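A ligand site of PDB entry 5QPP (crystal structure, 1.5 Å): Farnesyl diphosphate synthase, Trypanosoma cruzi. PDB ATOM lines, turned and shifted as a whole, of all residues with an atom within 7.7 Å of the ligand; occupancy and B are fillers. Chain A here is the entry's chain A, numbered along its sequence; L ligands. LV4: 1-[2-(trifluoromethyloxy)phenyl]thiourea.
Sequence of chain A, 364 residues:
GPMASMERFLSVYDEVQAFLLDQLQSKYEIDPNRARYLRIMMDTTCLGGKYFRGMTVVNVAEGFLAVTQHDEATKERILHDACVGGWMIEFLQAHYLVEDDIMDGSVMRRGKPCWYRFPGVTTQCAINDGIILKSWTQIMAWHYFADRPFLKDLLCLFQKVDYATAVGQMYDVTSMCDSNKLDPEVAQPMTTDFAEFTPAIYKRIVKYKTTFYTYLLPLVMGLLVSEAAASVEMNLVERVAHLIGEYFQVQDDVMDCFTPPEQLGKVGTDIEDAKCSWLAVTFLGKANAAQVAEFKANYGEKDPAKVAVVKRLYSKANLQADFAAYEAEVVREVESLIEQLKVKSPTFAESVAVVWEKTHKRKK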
ATOM      1  N   VAL A 250      -2.281  13.523  -0.607  1.00  0.00           N
ATOM      2  CA  VAL A 250      -0.984  14.029  -1.011  1.00  0.00           C
ATOM      3  C   VAL A 250       0.075  13.096  -0.519  1.00  0.00           C
ATOM      4  O   VAL A 250       1.006  12.741  -1.252  1.00  0.00           O
ATOM      5  CB  VAL A 250      -0.837  15.507  -0.575  1.00  0.00           C
ATOM      6  CG1 VAL A 250       0.563  16.024  -0.776  1.00  0.00           C
ATOM      7  CG2 VAL A 250      -1.754  16.366  -1.319  1.00  0.00           C
ATOM      8  N   GLN A 251      -0.012  12.671   0.735  1.00  0.00           N
ATOM      9  CA  GLN A 251       0.881  11.663   1.233  1.00  0.00           C
ATOM     10  C   GLN A 251       0.850  10.389   0.401  1.00  0.00           C
ATOM     11  O   GLN A 251       1.907   9.867   0.087  1.00  0.00           O
ATOM     12  CB  GLN A 251       0.544  11.278   2.675  1.00  0.00           C
ATOM     13  CG  GLN A 251       0.610  12.314   3.786  1.00  0.00           C
ATOM     14  CD  GLN A 251       0.049  11.763   5.076  1.00  0.00           C
ATOM     15  OE1 GLN A 251      -1.073  11.233   5.127  1.00  0.00           O
ATOM     16  NE2 GLN A 251       0.782  11.902   6.142  1.00  0.00           N
ATOM     17  N   ASP A 253       0.046  10.091  -2.759  1.00  0.00           N
ATOM     18  CA  ASP A 253       0.690  10.390  -4.037  1.00  0.00           C
ATOM     19  C   ASP A 253       2.204  10.405  -3.926  1.00  0.00           C
ATOM     20  O   ASP A 253       2.925   9.888  -4.808  1.00  0.00           O
ATOM     21  CB  ASP A 253       0.258  11.728  -4.648  1.00  0.00           C
ATOM     22  CG  ASP A 253      -1.167  11.741  -5.124  1.00  0.00           C
ATOM     23  OD1 ASP A 253      -1.828  10.638  -5.113  1.00  0.00           O
ATOM     24  OD2 ASP A 253      -1.634  12.890  -5.515  1.00  0.00           O
ATOM     25  N   VAL A 254       2.742  11.048  -2.934  1.00  0.00           N
ATOM     26  CA  VAL A 254       4.227  11.003  -2.753  1.00  0.00           C
ATOM     27  C   VAL A 254       4.701   9.593  -2.491  1.00  0.00           C
ATOM     28  O   VAL A 254       5.719   9.175  -3.009  1.00  0.00           O
ATOM     29  CB  VAL A 254       4.662  11.854  -1.573  1.00  0.00           C
ATOM     30  CG1 VAL A 254       6.142  11.591  -1.170  1.00  0.00           C
ATOM     31  CG2 VAL A 254       4.357  13.281  -1.855  1.00  0.00           C
ATOM     32  N   MET A 255       3.967   8.823  -1.724  1.00  0.00           N
ATOM     33  CA  MET A 255       4.435   7.422  -1.401  1.00  0.00           C
ATOM     34  C   MET A 255       4.441   6.521  -2.662  1.00  0.00           C
ATOM     35  O   MET A 255       5.301   5.678  -2.786  1.00  0.00           O
ATOM     36  CB  MET A 255       3.539   6.794  -0.343  1.00  0.00           C
ATOM     37  CG  MET A 255       3.733   7.442   1.042  1.00  0.00           C
ATOM     38  SD  MET A 255       2.891   6.462   2.335  1.00  0.00           S
ATOM     39  CE  MET A 255       1.318   7.297   2.434  1.00  0.00           C
ATOM     40  N   CYS A 257       5.210   7.243  -5.637  1.00  0.00           N
ATOM     41  CA  CYS A 257       6.386   7.500  -6.458  1.00  0.00           C
ATOM     42  C   CYS A 257       7.655   7.089  -5.643  1.00  0.00           C
ATOM     43  O   CYS A 257       8.570   6.429  -6.170  1.00  0.00           O
ATOM     44  CB  CYS A 257       6.438   8.950  -6.803  1.00  0.00           C
ATOM     45  SG  CYS A 257       7.860   9.408  -7.848  1.00  0.00           S
ATOM     46  N   PHE A 258       7.703   7.436  -4.349  1.00  0.00           N
ATOM     47  CA  PHE A 258       9.000   7.342  -3.590  1.00  0.00           C
ATOM     48  C   PHE A 258       9.122   6.288  -2.498  1.00  0.00           C
ATOM     49  O   PHE A 258      10.258   5.966  -2.117  1.00  0.00           O
ATOM     50  CB  PHE A 258       9.372   8.721  -3.058  1.00  0.00           C
ATOM     51  CG  PHE A 258       9.673   9.703  -4.129  1.00  0.00           C
ATOM     52  CD1 PHE A 258      10.766   9.520  -4.986  1.00  0.00           C
ATOM     53  CD2 PHE A 258       8.921  10.859  -4.267  1.00  0.00           C
ATOM     54  CE1 PHE A 258      11.088  10.489  -5.942  1.00  0.00           C
ATOM     55  CE2 PHE A 258       9.239  11.797  -5.232  1.00  0.00           C
ATOM     56  CZ  PHE A 258      10.331  11.625  -6.069  1.00  0.00           C
ATOM     57  N   THR A 259       8.034   5.652  -2.074  1.00  0.00           N
ATOM     58  CA  THR A 259       8.093   4.605  -1.035  1.00  0.00           C
ATOM     59  C   THR A 259       8.468   3.269  -1.725  1.00  0.00           C
ATOM     60  O   THR A 259       7.763   2.862  -2.638  1.00  0.00           O
ATOM     61  CB  THR A 259       6.766   4.465  -0.213  1.00  0.00           C
ATOM     62  OG1 THR A 259       6.525   5.640   0.570  1.00  0.00           O
ATOM     63  CG2 THR A 259       6.766   3.249   0.761  1.00  0.00           C
ATOM     64  N   TRP A 278      -0.217  14.952  -6.920  1.00  0.00           N
ATOM     65  CA  TRP A 278       0.317  16.167  -6.338  1.00  0.00           C
ATOM     66  C   TRP A 278       1.727  16.511  -6.878  1.00  0.00           C
ATOM     67  O   TRP A 278       2.075  17.654  -7.018  1.00  0.00           O
ATOM     68  CB  TRP A 278       0.345  16.042  -4.790  1.00  0.00           C
ATOM     69  CG  TRP A 278       0.888  17.241  -4.099  1.00  0.00           C
ATOM     70  CD1 TRP A 278       0.206  18.341  -3.751  1.00  0.00           C
ATOM     71  CD2 TRP A 278       2.256  17.461  -3.729  1.00  0.00           C
ATOM     72  NE1 TRP A 278       1.076  19.280  -3.167  1.00  0.00           N
ATOM     73  CE2 TRP A 278       2.321  18.728  -3.150  1.00  0.00           C
ATOM     74  CE3 TRP A 278       3.419  16.689  -3.834  1.00  0.00           C
ATOM     75  CZ2 TRP A 278       3.495  19.256  -2.676  1.00  0.00           C
ATOM     76  CZ3 TRP A 278       4.642  17.237  -3.388  1.00  0.00           C
ATOM     77  CH2 TRP A 278       4.639  18.495  -2.778  1.00  0.00           C
ATOM     78  N   LEU A 279       2.529  15.476  -7.076  1.00  0.00           N
ATOM     79  CA  LEU A 279       3.928  15.632  -7.547  1.00  0.00           C
ATOM     80  C   LEU A 279       3.896  16.286  -8.950  1.00  0.00           C
ATOM     81  O   LEU A 279       4.507  17.319  -9.139  1.00  0.00           O
ATOM     82  CB  LEU A 279       4.652  14.289  -7.612  1.00  0.00           C
ATOM     83  CG  LEU A 279       4.909  13.663  -6.222  1.00  0.00           C
ATOM     84  CD1 LEU A 279       5.264  12.171  -6.299  1.00  0.00           C
ATOM     85  CD2 LEU A 279       5.975  14.471  -5.527  1.00  0.00           C
ATOM     86  N   LYS A 311      11.006  10.786 -12.387  1.00  0.00           N
ATOM     87  CA  LYS A 311      11.394  10.793 -10.956  1.00  0.00           C
ATOM     88  C   LYS A 311      12.611  11.704 -10.687  1.00  0.00           C
ATOM     89  O   LYS A 311      12.631  12.501  -9.725  1.00  0.00           O
ATOM     90  CB  LYS A 311      11.662   9.400 -10.436  1.00  0.00           C
ATOM     91  CG  LYS A 311      10.417   8.479 -10.554  1.00  0.00           C
ATOM     92  CD  LYS A 311      10.436   7.397  -9.504  1.00  0.00           C
ATOM     93  CE  LYS A 311       9.327   6.359  -9.745  1.00  0.00           C
ATOM     94  NZ  LYS A 311       9.288   5.327  -8.719  1.00  0.00           N
ATOM     95  N   ARG A 312      13.602  11.585 -11.563  1.00  0.00           N
ATOM     96  CA  ARG A 312      14.754  12.516 -11.572  1.00  0.00           C
ATOM     97  C   ARG A 312      14.296  13.972 -11.674  1.00  0.00           C
ATOM     98  O   ARG A 312      14.814  14.870 -11.002  1.00  0.00           O
ATOM     99  CB  ARG A 312      15.696  12.188 -12.760  1.00  0.00           C
ATOM    100  CG  ARG A 312      17.133  12.760 -12.679  1.00  0.00           C
ATOM    101  CD  ARG A 312      18.044  12.009 -11.684  1.00  0.00           C
ATOM    102  NE  ARG A 312      17.877  10.530 -11.756  1.00  0.00           N
ATOM    103  CZ  ARG A 312      18.726   9.642 -12.302  1.00  0.00           C
ATOM    104  NH1 ARG A 312      19.900  10.012 -12.839  1.00  0.00           N
ATOM    105  NH2 ARG A 312      18.405   8.343 -12.296  1.00  0.00           N
ATOM    106  N   LEU A 313      13.334  14.260 -12.543  1.00  0.00           N
ATOM    107  CA  LEU A 313      12.858  15.644 -12.655  1.00  0.00           C
ATOM    108  C   LEU A 313      12.207  16.134 -11.334  1.00  0.00           C
ATOM    109  O   LEU A 313      12.419  17.318 -10.941  1.00  0.00           O
ATOM    110  CB  LEU A 313      11.879  15.794 -13.801  1.00  0.00           C
ATOM    111  CG  LEU A 313      12.285  15.904 -15.266  1.00  0.00           C
ATOM    112  CD1 LEU A 313      11.055  15.851 -16.147  1.00  0.00           C
ATOM    113  CD2 LEU A 313      13.109  17.149 -15.576  1.00  0.00           C
ATOM    114  N   TYR A 314      11.390  15.288 -10.703  1.00  0.00           N
ATOM    115  CA  TYR A 314      10.799  15.638  -9.411  1.00  0.00           C
ATOM    116  C   TYR A 314      11.868  15.889  -8.339  1.00  0.00           C
ATOM    117  O   TYR A 314      11.817  16.925  -7.690  1.00  0.00           O
ATOM    118  CB  TYR A 314       9.830  14.567  -8.892  1.00  0.00           C
ATOM    119  CG  TYR A 314       8.563  14.352  -9.694  1.00  0.00           C
ATOM    120  CD1 TYR A 314       8.073  15.310 -10.624  1.00  0.00           C
ATOM    121  CD2 TYR A 314       7.804  13.193  -9.467  1.00  0.00           C
ATOM    122  CE1 TYR A 314       6.906  15.059 -11.325  1.00  0.00           C
ATOM    123  CE2 TYR A 314       6.610  12.946 -10.157  1.00  0.00           C
ATOM    124  CZ  TYR A 314       6.183  13.885 -11.053  1.00  0.00           C
ATOM    125  OH  TYR A 314       5.034  13.705 -11.745  1.00  0.00           O
ATOM    126  N   SER A 315      12.814  14.964  -8.183  1.00  0.00           N
ATOM    127  CA  SER A 315      13.964  15.105  -7.210  1.00  0.00           C
ATOM    128  C   SER A 315      14.772  16.368  -7.485  1.00  0.00           C
ATOM    129  O   SER A 315      15.022  17.133  -6.549  1.00  0.00           O
ATOM    130  CB  SER A 315      14.891  13.863  -7.175  1.00  0.00           C
ATOM    131  OG  SER A 315      14.187  12.661  -6.967  1.00  0.00           O
ATOM    132  N   LYS A 316      15.155  16.634  -8.730  1.00  0.00           N
ATOM    133  CA  LYS A 316      15.855  17.933  -9.055  1.00  0.00           C
ATOM    134  C   LYS A 316      15.054  19.164  -8.698  1.00  0.00           C
ATOM    135  O   LYS A 316      15.627  20.228  -8.490  1.00  0.00           O
ATOM    136  CB  LYS A 316      16.227  18.077 -10.535  1.00  0.00           C
ATOM    137  CG  LYS A 316      17.567  17.489 -10.970  1.00  0.00           C
ATOM    138  CD  LYS A 316      17.669  17.416 -12.507  1.00  0.00           C
ATOM    139  CE  LYS A 316      18.682  16.361 -12.981  1.00  0.00           C
ATOM    140  NZ  LYS A 316      18.269  15.708 -14.269  1.00  0.00           N
ATOM    141  N   ALA A 317      13.722  19.060  -8.686  1.00  0.00           N
ATOM    142  CA  ALA A 317      12.844  20.184  -8.438  1.00  0.00           C
ATOM    143  C   ALA A 317      12.578  20.431  -6.932  1.00  0.00           C
ATOM    144  O   ALA A 317      11.900  21.403  -6.612  1.00  0.00           O
ATOM    145  CB  ALA A 317      11.502  19.973  -9.170  1.00  0.00           C
ATOM    146  N   ASN A 318      13.134  19.570  -6.075  1.00  0.00           N
ATOM    147  CA  ASN A 318      13.063  19.692  -4.629  1.00  0.00           C
ATOM    148  C   ASN A 318      11.569  19.907  -4.227  1.00  0.00           C
ATOM    149  O   ASN A 318      11.163  20.872  -3.625  1.00  0.00           O
ATOM    150  CB  ASN A 318      13.920  20.835  -4.123  1.00  0.00           C
ATOM    151  CG  ASN A 318      14.125  20.792  -2.599  1.00  0.00           C
ATOM    152  OD1 ASN A 318      14.555  21.789  -2.019  1.00  0.00           O
ATOM    153  ND2 ASN A 318      13.835  19.632  -1.940  1.00  0.00           N
ATOM    154  N   LEU A 319      10.751  18.981  -4.668  1.00  0.00           N
ATOM    155  CA  LEU A 319       9.374  18.910  -4.240  1.00  0.00           C
ATOM    156  C   LEU A 319       9.230  18.647  -2.736  1.00  0.00           C
ATOM    157  O   LEU A 319       8.197  18.998  -2.163  1.00  0.00           O
ATOM    158  CB  LEU A 319       8.612  17.848  -5.073  1.00  0.00           C
ATOM    159  CG  LEU A 319       8.604  18.158  -6.590  1.00  0.00           C
ATOM    160  CD1 LEU A 319       7.870  17.004  -7.266  1.00  0.00           C
ATOM    161  CD2 LEU A 319       7.985  19.476  -6.923  1.00  0.00           C
ATOM    162  N   GLN A 320      10.227  18.020  -2.096  1.00  0.00           N
ATOM    163  CA  GLN A 320      10.258  17.935  -0.615  1.00  0.00           C
ATOM    164  C   GLN A 320       9.978  19.274   0.064  1.00  0.00           C
ATOM    165  O   GLN A 320       9.202  19.334   1.028  1.00  0.00           O
ATOM    166  CB  GLN A 320      11.612  17.383  -0.085  1.00  0.00           C
ATOM    167  CG  GLN A 320      11.572  15.890   0.257  1.00  0.00           C
ATOM    168  CD  GLN A 320      12.622  15.430   1.258  1.00  0.00           C
ATOM    169  OE1 GLN A 320      13.036  14.260   1.242  1.00  0.00           O
ATOM    170  NE2 GLN A 320      13.040  16.319   2.163  1.00  0.00           N
ATOM    171  N   ALA A 321      10.577  20.346  -0.441  1.00  0.00           N
ATOM    172  CA  ALA A 321      10.320  21.681   0.140  1.00  0.00           C
ATOM    173  C   ALA A 321       8.906  22.210  -0.152  1.00  0.00           C
ATOM    174  O   ALA A 321       8.314  22.913   0.679  1.00  0.00           O
ATOM    175  CB  ALA A 321      11.372  22.681  -0.291  1.00  0.00           C
ATOM    176  N   ASP A 322       8.349  21.892  -1.322  1.00  0.00           N
ATOM    177  CA  ASP A 322       6.968  22.337  -1.553  1.00  0.00           C
ATOM    178  C   ASP A 322       6.062  21.559  -0.588  1.00  0.00           C
ATOM    179  O   ASP A 322       5.034  22.093  -0.106  1.00  0.00           O
ATOM    180  CB  ASP A 322       6.559  22.022  -2.959  1.00  0.00           C
ATOM    181  CG  ASP A 322       7.309  22.841  -3.970  1.00  0.00           C
ATOM    182  OD1 ASP A 322       8.335  22.328  -4.411  1.00  0.00           O
ATOM    183  OD2 ASP A 322       6.827  23.936  -4.318  1.00  0.00           O
ATOM    184  N   PHE A 323       6.423  20.303  -0.358  1.00  0.00           N
ATOM    185  CA  PHE A 323       5.601  19.414   0.498  1.00  0.00           C
ATOM    186  C   PHE A 323       5.628  19.910   1.959  1.00  0.00           C
ATOM    187  O   PHE A 323       4.600  19.907   2.634  1.00  0.00           O
ATOM    188  CB  PHE A 323       6.032  17.938   0.508  1.00  0.00           C
ATOM    189  CG  PHE A 323       5.196  17.106   1.460  1.00  0.00           C
ATOM    190  CD1 PHE A 323       3.929  16.603   1.069  1.00  0.00           C
ATOM    191  CD2 PHE A 323       5.623  16.879   2.759  1.00  0.00           C
ATOM    192  CE1 PHE A 323       3.168  15.886   1.959  1.00  0.00           C
ATOM    193  CE2 PHE A 323       4.838  16.178   3.640  1.00  0.00           C
ATOM    194  CZ  PHE A 323       3.646  15.652   3.244  1.00  0.00           C
ATOM    195  N   ALA A 324       6.818  20.252   2.437  1.00  0.00           N
ATOM    196  CA  ALA A 324       6.959  20.769   3.807  1.00  0.00           C
ATOM    197  C   ALA A 324       6.124  22.028   3.981  1.00  0.00           C
ATOM    198  O   ALA A 324       5.483  22.223   5.018  1.00  0.00           O
ATOM    199  CB  ALA A 324       8.436  20.972   4.161  1.00  0.00           C
HETATM  200  N1  LV4 L   1      12.530  12.795  -4.059  1.00  0.00           N
HETATM  201  C4  LV4 L   1       9.720  13.815  -1.892  1.00  0.00           C
HETATM  202  C5  LV4 L   1       8.762  14.674  -2.502  1.00  0.00           C
HETATM  203  C6  LV4 L   1      11.542  13.630  -3.660  1.00  0.00           C
HETATM  204  C7  LV4 L   1      10.356  11.403   0.328  1.00  0.00           C
HETATM  205  N   LV4 L   1      10.815  13.189  -2.564  1.00  0.00           N
HETATM  206  C   LV4 L   1       7.695  15.171  -1.765  1.00  0.00           C
HETATM  207  O   LV4 L   1      10.509  12.773   0.163  1.00  0.00           O
HETATM  208  C1  LV4 L   1       7.535  14.828  -0.416  1.00  0.00           C
HETATM  209  C2  LV4 L   1       8.449  13.993   0.218  1.00  0.00           C
HETATM  210  C3  LV4 L   1       9.547  13.512  -0.510  1.00  0.00           C
HETATM  211  F   LV4 L   1       9.334  11.200   1.195  1.00  0.00           F
HETATM  212  F1  LV4 L   1      11.429  10.859   0.848  1.00  0.00           F
HETATM  213  F2  LV4 L   1      10.126  10.766  -0.827  1.00  0.00           F
HETATM  214  S   LV4 L   1      11.353  14.999  -4.542  1.00  0.00           S
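OE1 of Gln 320 lies close to O of the ligand (3.1 Å).
OG of Ser 315 lies within hydrogen-bond range of N1 of the ligand (3.3 Å).
The side-chain hydroxyl (OG) of Ser 315 lies within hydrogen-bond range of the backbone carbonyl oxygen (O) of Lys 311 (3.2 Å).
O of Tyr 314 lies close to S of the ligand (3.7 Å).
Val 254 touches the ligand (CG1 to C1, 3.6 Å).
CB of Phe 258 touches F2 of the ligand, at 3.1 Å.
Leu 319 touches the ligand (O to C, 3.9 Å).
Phe 323 touches the ligand.
Seven residues have an atom within 4 Å of the ligand: Val 254, Phe 258, Tyr 314, Ser 315, Leu 319, Gln 320 and Phe 323.
The nearest printed residue that does not touch the ligand is Trp 278 (4.03 Å).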
